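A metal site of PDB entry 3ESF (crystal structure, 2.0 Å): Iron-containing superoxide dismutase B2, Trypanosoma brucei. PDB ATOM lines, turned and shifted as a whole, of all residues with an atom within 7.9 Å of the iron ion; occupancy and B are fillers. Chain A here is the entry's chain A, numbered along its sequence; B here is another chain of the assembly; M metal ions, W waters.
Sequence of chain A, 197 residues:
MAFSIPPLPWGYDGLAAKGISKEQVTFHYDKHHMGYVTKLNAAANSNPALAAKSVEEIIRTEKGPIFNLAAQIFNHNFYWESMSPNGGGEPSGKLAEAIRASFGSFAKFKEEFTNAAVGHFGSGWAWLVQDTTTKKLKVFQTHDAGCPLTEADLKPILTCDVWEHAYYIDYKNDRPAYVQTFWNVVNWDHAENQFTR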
ATOM      1  N   HIS A  28       9.541  11.874  20.414  1.00  0.00           N
ATOM      2  CA  HIS A  28       8.917  12.404  19.212  1.00  0.00           C
ATOM      3  C   HIS A  28       9.895  12.462  18.006  1.00  0.00           C
ATOM      4  O   HIS A  28       9.562  12.043  16.880  1.00  0.00           O
ATOM      5  CB  HIS A  28       8.306  13.779  19.523  1.00  0.00           C
ATOM      6  CG  HIS A  28       7.317  14.227  18.515  1.00  0.00           C
ATOM      7  ND1 HIS A  28       6.710  15.459  18.576  1.00  0.00           N
ATOM      8  CD2 HIS A  28       6.837  13.620  17.403  1.00  0.00           C
ATOM      9  CE1 HIS A  28       5.896  15.594  17.539  1.00  0.00           C
ATOM     10  NE2 HIS A  28       5.955  14.498  16.818  1.00  0.00           N
ATOM     11  N   TYR A  29      11.098  12.960  18.296  1.00  0.00           N
ATOM     12  CA  TYR A  29      12.154  13.049  17.300  1.00  0.00           C
ATOM     13  C   TYR A  29      12.804  11.682  17.048  1.00  0.00           C
ATOM     14  O   TYR A  29      12.858  11.259  15.899  1.00  0.00           O
ATOM     15  CB  TYR A  29      13.229  14.110  17.689  1.00  0.00           C
ATOM     16  CG  TYR A  29      14.296  14.365  16.632  1.00  0.00           C
ATOM     17  CD1 TYR A  29      14.139  15.401  15.695  1.00  0.00           C
ATOM     18  CD2 TYR A  29      15.457  13.590  16.585  1.00  0.00           C
ATOM     19  CE1 TYR A  29      15.114  15.641  14.717  1.00  0.00           C
ATOM     20  CE2 TYR A  29      16.413  13.794  15.618  1.00  0.00           C
ATOM     21  CZ  TYR A  29      16.243  14.834  14.677  1.00  0.00           C
ATOM     22  OH  TYR A  29      17.228  15.053  13.727  1.00  0.00           O
ATOM     23  N   HIS A  32       9.343   8.675  16.494  1.00  0.00           N
ATOM     24  CA  HIS A  32       8.399   8.986  15.422  1.00  0.00           C
ATOM     25  C   HIS A  32       9.042   9.605  14.195  1.00  0.00           C
ATOM     26  O   HIS A  32       8.920   9.039  13.103  1.00  0.00           O
ATOM     27  CB  HIS A  32       7.196   9.826  15.904  1.00  0.00           C
ATOM     28  CG  HIS A  32       6.414   9.128  16.968  1.00  0.00           C
ATOM     29  ND1 HIS A  32       5.485   8.148  16.691  1.00  0.00           N
ATOM     30  CD2 HIS A  32       6.491   9.200  18.323  1.00  0.00           C
ATOM     31  CE1 HIS A  32       4.988   7.685  17.822  1.00  0.00           C
ATOM     32  NE2 HIS A  32       5.593   8.296  18.835  1.00  0.00           N
ATOM     33  N   HIS A  33       9.725  10.730  14.365  1.00  0.00           N
ATOM     34  CA  HIS A  33      10.289  11.503  13.259  1.00  0.00           C
ATOM     35  C   HIS A  33      11.366  10.684  12.538  1.00  0.00           C
ATOM     36  O   HIS A  33      11.279  10.466  11.314  1.00  0.00           O
ATOM     37  CB  HIS A  33      10.802  12.898  13.735  1.00  0.00           C
ATOM     38  CG  HIS A  33      11.139  13.859  12.628  1.00  0.00           C
ATOM     39  ND1 HIS A  33      11.708  15.096  12.845  1.00  0.00           N
ATOM     40  CD2 HIS A  33      11.016  13.758  11.276  1.00  0.00           C
ATOM     41  CE1 HIS A  33      11.916  15.708  11.693  1.00  0.00           C
ATOM     42  NE2 HIS A  33      11.502  14.905  10.725  1.00  0.00           N
ATOM     43  N   TYR A  36      10.104   7.562  10.450  1.00  0.00           N
ATOM     44  CA  TYR A  36       9.695   7.807   9.066  1.00  0.00           C
ATOM     45  C   TYR A  36      10.881   7.751   8.108  1.00  0.00           C
ATOM     46  O   TYR A  36      10.777   7.181   7.027  1.00  0.00           O
ATOM     47  CB  TYR A  36       8.964   9.157   8.912  1.00  0.00           C
ATOM     48  CG  TYR A  36       7.682   9.283   9.732  1.00  0.00           C
ATOM     49  CD1 TYR A  36       6.613   8.414   9.519  1.00  0.00           C
ATOM     50  CD2 TYR A  36       7.530  10.292  10.694  1.00  0.00           C
ATOM     51  CE1 TYR A  36       5.424   8.504  10.270  1.00  0.00           C
ATOM     52  CE2 TYR A  36       6.344  10.404  11.456  1.00  0.00           C
ATOM     53  CZ  TYR A  36       5.294   9.495  11.218  1.00  0.00           C
ATOM     54  OH  TYR A  36       4.121   9.598  11.949  1.00  0.00           O
ATOM     55  N   GLN A  72       5.261  13.345   6.408  1.00  0.00           N
ATOM     56  CA  GLN A  72       5.564  13.408   7.837  1.00  0.00           C
ATOM     57  C   GLN A  72       6.975  13.902   8.130  1.00  0.00           C
ATOM     58  O   GLN A  72       7.187  14.595   9.113  1.00  0.00           O
ATOM     59  CB  GLN A  72       5.337  12.073   8.521  1.00  0.00           C
ATOM     60  CG  GLN A  72       3.872  11.695   8.636  1.00  0.00           C
ATOM     61  CD  GLN A  72       3.112  12.559   9.611  1.00  0.00           C
ATOM     62  OE1 GLN A  72       2.600  13.609   9.250  1.00  0.00           O
ATOM     63  NE2 GLN A  72       3.037  12.113  10.861  1.00  0.00           N
ATOM     64  N   ASN A  75       6.729  17.691   7.520  1.00  0.00           N
ATOM     65  CA  ASN A  75       5.847  18.281   8.539  1.00  0.00           C
ATOM     66  C   ASN A  75       6.572  18.404   9.879  1.00  0.00           C
ATOM     67  O   ASN A  75       6.451  19.412  10.531  1.00  0.00           O
ATOM     68  CB  ASN A  75       4.565  17.457   8.735  1.00  0.00           C
ATOM     69  CG  ASN A  75       3.615  17.543   7.545  1.00  0.00           C
ATOM     70  OD1 ASN A  75       3.770  18.373   6.639  1.00  0.00           O
ATOM     71  ND2 ASN A  75       2.637  16.669   7.545  1.00  0.00           N
ATOM     72  N   HIS A  76       7.300  17.364  10.286  1.00  0.00           N
ATOM     73  CA  HIS A  76       8.054  17.394  11.549  1.00  0.00           C
ATOM     74  C   HIS A  76       9.216  18.349  11.521  1.00  0.00           C
ATOM     75  O   HIS A  76       9.500  19.002  12.506  1.00  0.00           O
ATOM     76  CB  HIS A  76       8.523  15.991  11.929  1.00  0.00           C
ATOM     77  CG  HIS A  76       7.421  15.123  12.448  1.00  0.00           C
ATOM     78  ND1 HIS A  76       6.534  14.480  11.615  1.00  0.00           N
ATOM     79  CD2 HIS A  76       7.020  14.873  13.711  1.00  0.00           C
ATOM     80  CE1 HIS A  76       5.638  13.848  12.352  1.00  0.00           C
ATOM     81  NE2 HIS A  76       5.893  14.101  13.627  1.00  0.00           N
ATOM     82  N   TYR A  79       7.605  21.671  11.886  1.00  0.00           N
ATOM     83  CA  TYR A  79       7.173  21.743  13.290  1.00  0.00           C
ATOM     84  C   TYR A  79       8.272  22.163  14.283  1.00  0.00           C
ATOM     85  O   TYR A  79       8.045  23.055  15.090  1.00  0.00           O
ATOM     86  CB  TYR A  79       6.616  20.374  13.694  1.00  0.00           C
ATOM     87  CG  TYR A  79       6.202  20.217  15.142  1.00  0.00           C
ATOM     88  CD1 TYR A  79       5.268  21.082  15.731  1.00  0.00           C
ATOM     89  CD2 TYR A  79       6.744  19.178  15.928  1.00  0.00           C
ATOM     90  CE1 TYR A  79       4.855  20.907  17.050  1.00  0.00           C
ATOM     91  CE2 TYR A  79       6.363  19.003  17.240  1.00  0.00           C
ATOM     92  CZ  TYR A  79       5.395  19.853  17.802  1.00  0.00           C
ATOM     93  OH  TYR A  79       5.009  19.659  19.116  1.00  0.00           O
ATOM     94  N   TRP A  80       9.428  21.498  14.264  1.00  0.00           N
ATOM     95  CA  TRP A  80      10.528  21.861  15.150  1.00  0.00           C
ATOM     96  C   TRP A  80      10.990  23.289  14.899  1.00  0.00           C
ATOM     97  O   TRP A  80      11.269  24.011  15.853  1.00  0.00           O
ATOM     98  CB  TRP A  80      11.747  20.907  15.065  1.00  0.00           C
ATOM     99  CG  TRP A  80      11.453  19.472  15.297  1.00  0.00           C
ATOM    100  CD1 TRP A  80      11.757  18.429  14.464  1.00  0.00           C
ATOM    101  CD2 TRP A  80      10.791  18.887  16.431  1.00  0.00           C
ATOM    102  NE1 TRP A  80      11.312  17.247  15.002  1.00  0.00           N
ATOM    103  CE2 TRP A  80      10.721  17.490  16.202  1.00  0.00           C
ATOM    104  CE3 TRP A  80      10.250  19.409  17.629  1.00  0.00           C
ATOM    105  CZ2 TRP A  80      10.136  16.602  17.121  1.00  0.00           C
ATOM    106  CZ3 TRP A  80       9.663  18.530  18.538  1.00  0.00           C
ATOM    107  CH2 TRP A  80       9.615  17.134  18.284  1.00  0.00           C
ATOM    108  N   GLY A 124      -3.580  14.825  13.151  1.00  0.00           N
ATOM    109  CA  GLY A 124      -3.343  15.890  12.141  1.00  0.00           C
ATOM    110  C   GLY A 124      -2.468  17.062  12.558  1.00  0.00           C
ATOM    111  O   GLY A 124      -1.667  16.968  13.488  1.00  0.00           O
ATOM    112  N   TRP A 125      -2.620  18.194  11.854  1.00  0.00           N
ATOM    113  CA  TRP A 125      -1.682  19.313  11.883  1.00  0.00           C
ATOM    114  C   TRP A 125      -2.487  20.600  11.725  1.00  0.00           C
ATOM    115  O   TRP A 125      -3.361  20.670  10.851  1.00  0.00           O
ATOM    116  CB  TRP A 125      -0.695  19.228  10.716  1.00  0.00           C
ATOM    117  CG  TRP A 125       0.143  18.013  10.703  1.00  0.00           C
ATOM    118  CD1 TRP A 125      -0.200  16.785  10.186  1.00  0.00           C
ATOM    119  CD2 TRP A 125       1.456  17.896  11.219  1.00  0.00           C
ATOM    120  NE1 TRP A 125       0.828  15.895  10.392  1.00  0.00           N
ATOM    121  CE2 TRP A 125       1.861  16.542  11.020  1.00  0.00           C
ATOM    122  CE3 TRP A 125       2.342  18.782  11.846  1.00  0.00           C
ATOM    123  CZ2 TRP A 125       3.102  16.070  11.409  1.00  0.00           C
ATOM    124  CZ3 TRP A 125       3.599  18.291  12.272  1.00  0.00           C
ATOM    125  CH2 TRP A 125       3.945  16.949  12.050  1.00  0.00           C
ATOM    126  N   ASP A 161       1.944  20.231  15.426  1.00  0.00           N
ATOM    127  CA  ASP A 161       1.598  18.802  15.386  1.00  0.00           C
ATOM    128  C   ASP A 161       0.544  18.544  16.447  1.00  0.00           C
ATOM    129  O   ASP A 161       0.773  18.901  17.599  1.00  0.00           O
ATOM    130  CB  ASP A 161       2.858  17.937  15.698  1.00  0.00           C
ATOM    131  CG  ASP A 161       2.692  16.469  15.374  1.00  0.00           C
ATOM    132  OD1 ASP A 161       1.616  16.065  14.893  1.00  0.00           O
ATOM    133  OD2 ASP A 161       3.676  15.680  15.549  1.00  0.00           O
ATOM    134  N   VAL A 162      -0.591  17.960  16.056  1.00  0.00           N
ATOM    135  CA  VAL A 162      -1.619  17.561  17.063  1.00  0.00           C
ATOM    136  C   VAL A 162      -1.952  16.059  17.049  1.00  0.00           C
ATOM    137  O   VAL A 162      -2.961  15.624  17.624  1.00  0.00           O
ATOM    138  CB  VAL A 162      -2.906  18.439  17.002  1.00  0.00           C
ATOM    139  CG1 VAL A 162      -2.561  19.886  17.230  1.00  0.00           C
ATOM    140  CG2 VAL A 162      -3.681  18.236  15.667  1.00  0.00           C
ATOM    141  N   TRP A 163      -1.114  15.251  16.390  1.00  0.00           N
ATOM    142  CA  TRP A 163      -1.094  13.824  16.690  1.00  0.00           C
ATOM    143  C   TRP A 163      -0.854  13.675  18.201  1.00  0.00           C
ATOM    144  O   TRP A 163      -0.048  14.438  18.769  1.00  0.00           O
ATOM    145  CB  TRP A 163       0.084  13.125  15.981  1.00  0.00           C
ATOM    146  CG  TRP A 163      -0.072  12.888  14.495  1.00  0.00           C
ATOM    147  CD1 TRP A 163      -0.318  13.837  13.505  1.00  0.00           C
ATOM    148  CD2 TRP A 163       0.057  11.634  13.823  1.00  0.00           C
ATOM    149  NE1 TRP A 163      -0.364  13.209  12.273  1.00  0.00           N
ATOM    150  CE2 TRP A 163      -0.146  11.865  12.444  1.00  0.00           C
ATOM    151  CE3 TRP A 163       0.324  10.326  14.257  1.00  0.00           C
ATOM    152  CZ2 TRP A 163      -0.085  10.817  11.477  1.00  0.00           C
ATOM    153  CZ3 TRP A 163       0.374   9.296  13.321  1.00  0.00           C
ATOM    154  CH2 TRP A 163       0.186   9.553  11.933  1.00  0.00           C
ATOM    155  N   GLU A 164      -1.493  12.683  18.811  1.00  0.00           N
ATOM    156  CA  GLU A 164      -1.421  12.472  20.223  1.00  0.00           C
ATOM    157  C   GLU A 164       0.001  12.284  20.741  1.00  0.00           C
ATOM    158  O   GLU A 164       0.290  12.693  21.859  1.00  0.00           O
ATOM    159  CB  GLU A 164      -2.349  11.348  20.678  1.00  0.00           C
ATOM    160  CG  GLU A 164      -3.789  11.817  20.689  1.00  0.00           C
ATOM    161  CD  GLU A 164      -4.829  10.729  20.898  1.00  0.00           C
ATOM    162  OE1 GLU A 164      -4.607   9.570  20.544  1.00  0.00           O
ATOM    163  OE2 GLU A 164      -5.900  11.038  21.431  1.00  0.00           O
ATOM    164  N   HIS A 165       0.873  11.645  19.937  1.00  0.00           N
ATOM    165  CA  HIS A 165       2.272  11.446  20.341  1.00  0.00           C
ATOM    166  C   HIS A 165       3.082  12.737  20.520  1.00  0.00           C
ATOM    167  O   HIS A 165       4.120  12.719  21.191  1.00  0.00           O
ATOM    168  CB  HIS A 165       3.014  10.477  19.399  1.00  0.00           C
ATOM    169  CG  HIS A 165       3.291  11.019  18.040  1.00  0.00           C
ATOM    170  ND1 HIS A 165       2.867  10.401  16.884  1.00  0.00           N
ATOM    171  CD2 HIS A 165       3.953  12.130  17.639  1.00  0.00           C
ATOM    172  CE1 HIS A 165       3.280  11.076  15.831  1.00  0.00           C
ATOM    173  NE2 HIS A 165       3.926  12.157  16.268  1.00  0.00           N
ATOM    174  N   ALA A 166       2.623  13.833  19.917  1.00  0.00           N
ATOM    175  CA  ALA A 166       3.260  15.126  20.072  1.00  0.00           C
ATOM    176  C   ALA A 166       3.168  15.634  21.513  1.00  0.00           C
ATOM    177  O   ALA A 166       4.060  16.378  21.971  1.00  0.00           O
ATOM    178  CB  ALA A 166       2.681  16.140  19.120  1.00  0.00           C
ATOM    179  N   TYR A 167       2.129  15.239  22.236  1.00  0.00           N
ATOM    180  CA  TYR A 167       1.858  15.869  23.531  1.00  0.00           C
ATOM    181  C   TYR A 167       1.534  14.886  24.653  1.00  0.00           C
ATOM    182  O   TYR A 167       1.447  15.309  25.809  1.00  0.00           O
ATOM    183  CB  TYR A 167       0.763  16.934  23.392  1.00  0.00           C
ATOM    184  CG  TYR A 167      -0.567  16.421  22.840  1.00  0.00           C
ATOM    185  CD1 TYR A 167      -1.509  15.831  23.699  1.00  0.00           C
ATOM    186  CD2 TYR A 167      -0.895  16.521  21.475  1.00  0.00           C
ATOM    187  CE1 TYR A 167      -2.737  15.346  23.238  1.00  0.00           C
ATOM    188  CE2 TYR A 167      -2.157  16.052  20.988  1.00  0.00           C
ATOM    189  CZ  TYR A 167      -3.050  15.458  21.911  1.00  0.00           C
ATOM    190  OH  TYR A 167      -4.282  14.986  21.534  1.00  0.00           O
ATOM    191  N   TYR A 178      -1.503  21.736  25.928  1.00  0.00           N
ATOM    192  CA  TYR A 178      -0.402  21.616  24.949  1.00  0.00           C
ATOM    193  C   TYR A 178      -0.418  22.810  23.989  1.00  0.00           C
ATOM    194  O   TYR A 178       0.627  23.418  23.733  1.00  0.00           O
ATOM    195  CB  TYR A 178      -0.482  20.283  24.202  1.00  0.00           C
ATOM    196  CG  TYR A 178       0.295  20.193  22.893  1.00  0.00           C
ATOM    197  CD1 TYR A 178       1.706  20.264  22.875  1.00  0.00           C
ATOM    198  CD2 TYR A 178      -0.371  19.988  21.679  1.00  0.00           C
ATOM    199  CE1 TYR A 178       2.429  20.174  21.680  1.00  0.00           C
ATOM    200  CE2 TYR A 178       0.332  19.892  20.473  1.00  0.00           C
ATOM    201  CZ  TYR A 178       1.729  19.972  20.487  1.00  0.00           C
ATOM    202  OH  TYR A 178       2.420  19.894  19.312  1.00  0.00           O
ATOM    203  N   GLU B 164      -3.305   6.474  19.354  1.00  0.00           N
ATOM    204  CA  GLU B 164      -2.126   6.593  20.235  1.00  0.00           C
ATOM    205  C   GLU B 164      -2.447   6.671  21.736  1.00  0.00           C
ATOM    206  O   GLU B 164      -1.735   6.079  22.534  1.00  0.00           O
ATOM    207  CB  GLU B 164      -1.223   7.739  19.806  1.00  0.00           C
ATOM    208  CG  GLU B 164      -0.659   7.437  18.435  1.00  0.00           C
ATOM    209  CD  GLU B 164       0.247   8.490  17.886  1.00  0.00           C
ATOM    210  OE1 GLU B 164      -0.097   9.701  17.929  1.00  0.00           O
ATOM    211  OE2 GLU B 164       1.293   8.088  17.308  1.00  0.00           O
HETATM  212 FE    FE M   1       4.517  13.924  15.280  1.00  0.00          FE
HETATM  213  O   HOH W   1       2.962  13.656  13.829  1.00  0.00           O
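The backbone NH of Trp 163 sits at hydrogen-bond distance from the side-chain carboxylate of Asp 161, at 3.2 Å.
O of Asp 161 is in hydrogen-bond range of OH of Tyr 178 (2.6 Å).
A ring nitrogen (ND1) of His 165 sits at hydrogen-bond distance from a ring nitrogen (ND1) of His 32, at 3.5 Å.
A ring nitrogen (ND1) of His 165 sits at hydrogen-bond distance from the side-chain carboxylate (OE2) of Glu 164 of chain B, at 2.8 Å.
ND1 of His 76 is in hydrogen-bond range of O of Gln 72, 2.6 Å away.
The backbone carbonyl oxygen of His 28 sits at hydrogen-bond distance from the backbone NH of His 33, 2.8 Å away.
Of the 21 residues printed, 4 come within 4 Å of the iron ion.
OD2 of Asp 161 is bound to the iron ion (2.0 Å).
NE2 of His 165 binds the iron ion (2.1 Å).
The iron ion is bound by water W1 (2.1 Å).
The iron ion is bound by a ring nitrogen (NE2) of His 76 (2.2 Å).
The iron ion is bound by a ring nitrogen (NE2) of His 28, 2.2 Å away.
Water W1 bridges the side-chain carboxylate of Asp 161 (3.0 Å) and the side-chain amide nitrogen of Gln 72 (3.3 Å).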
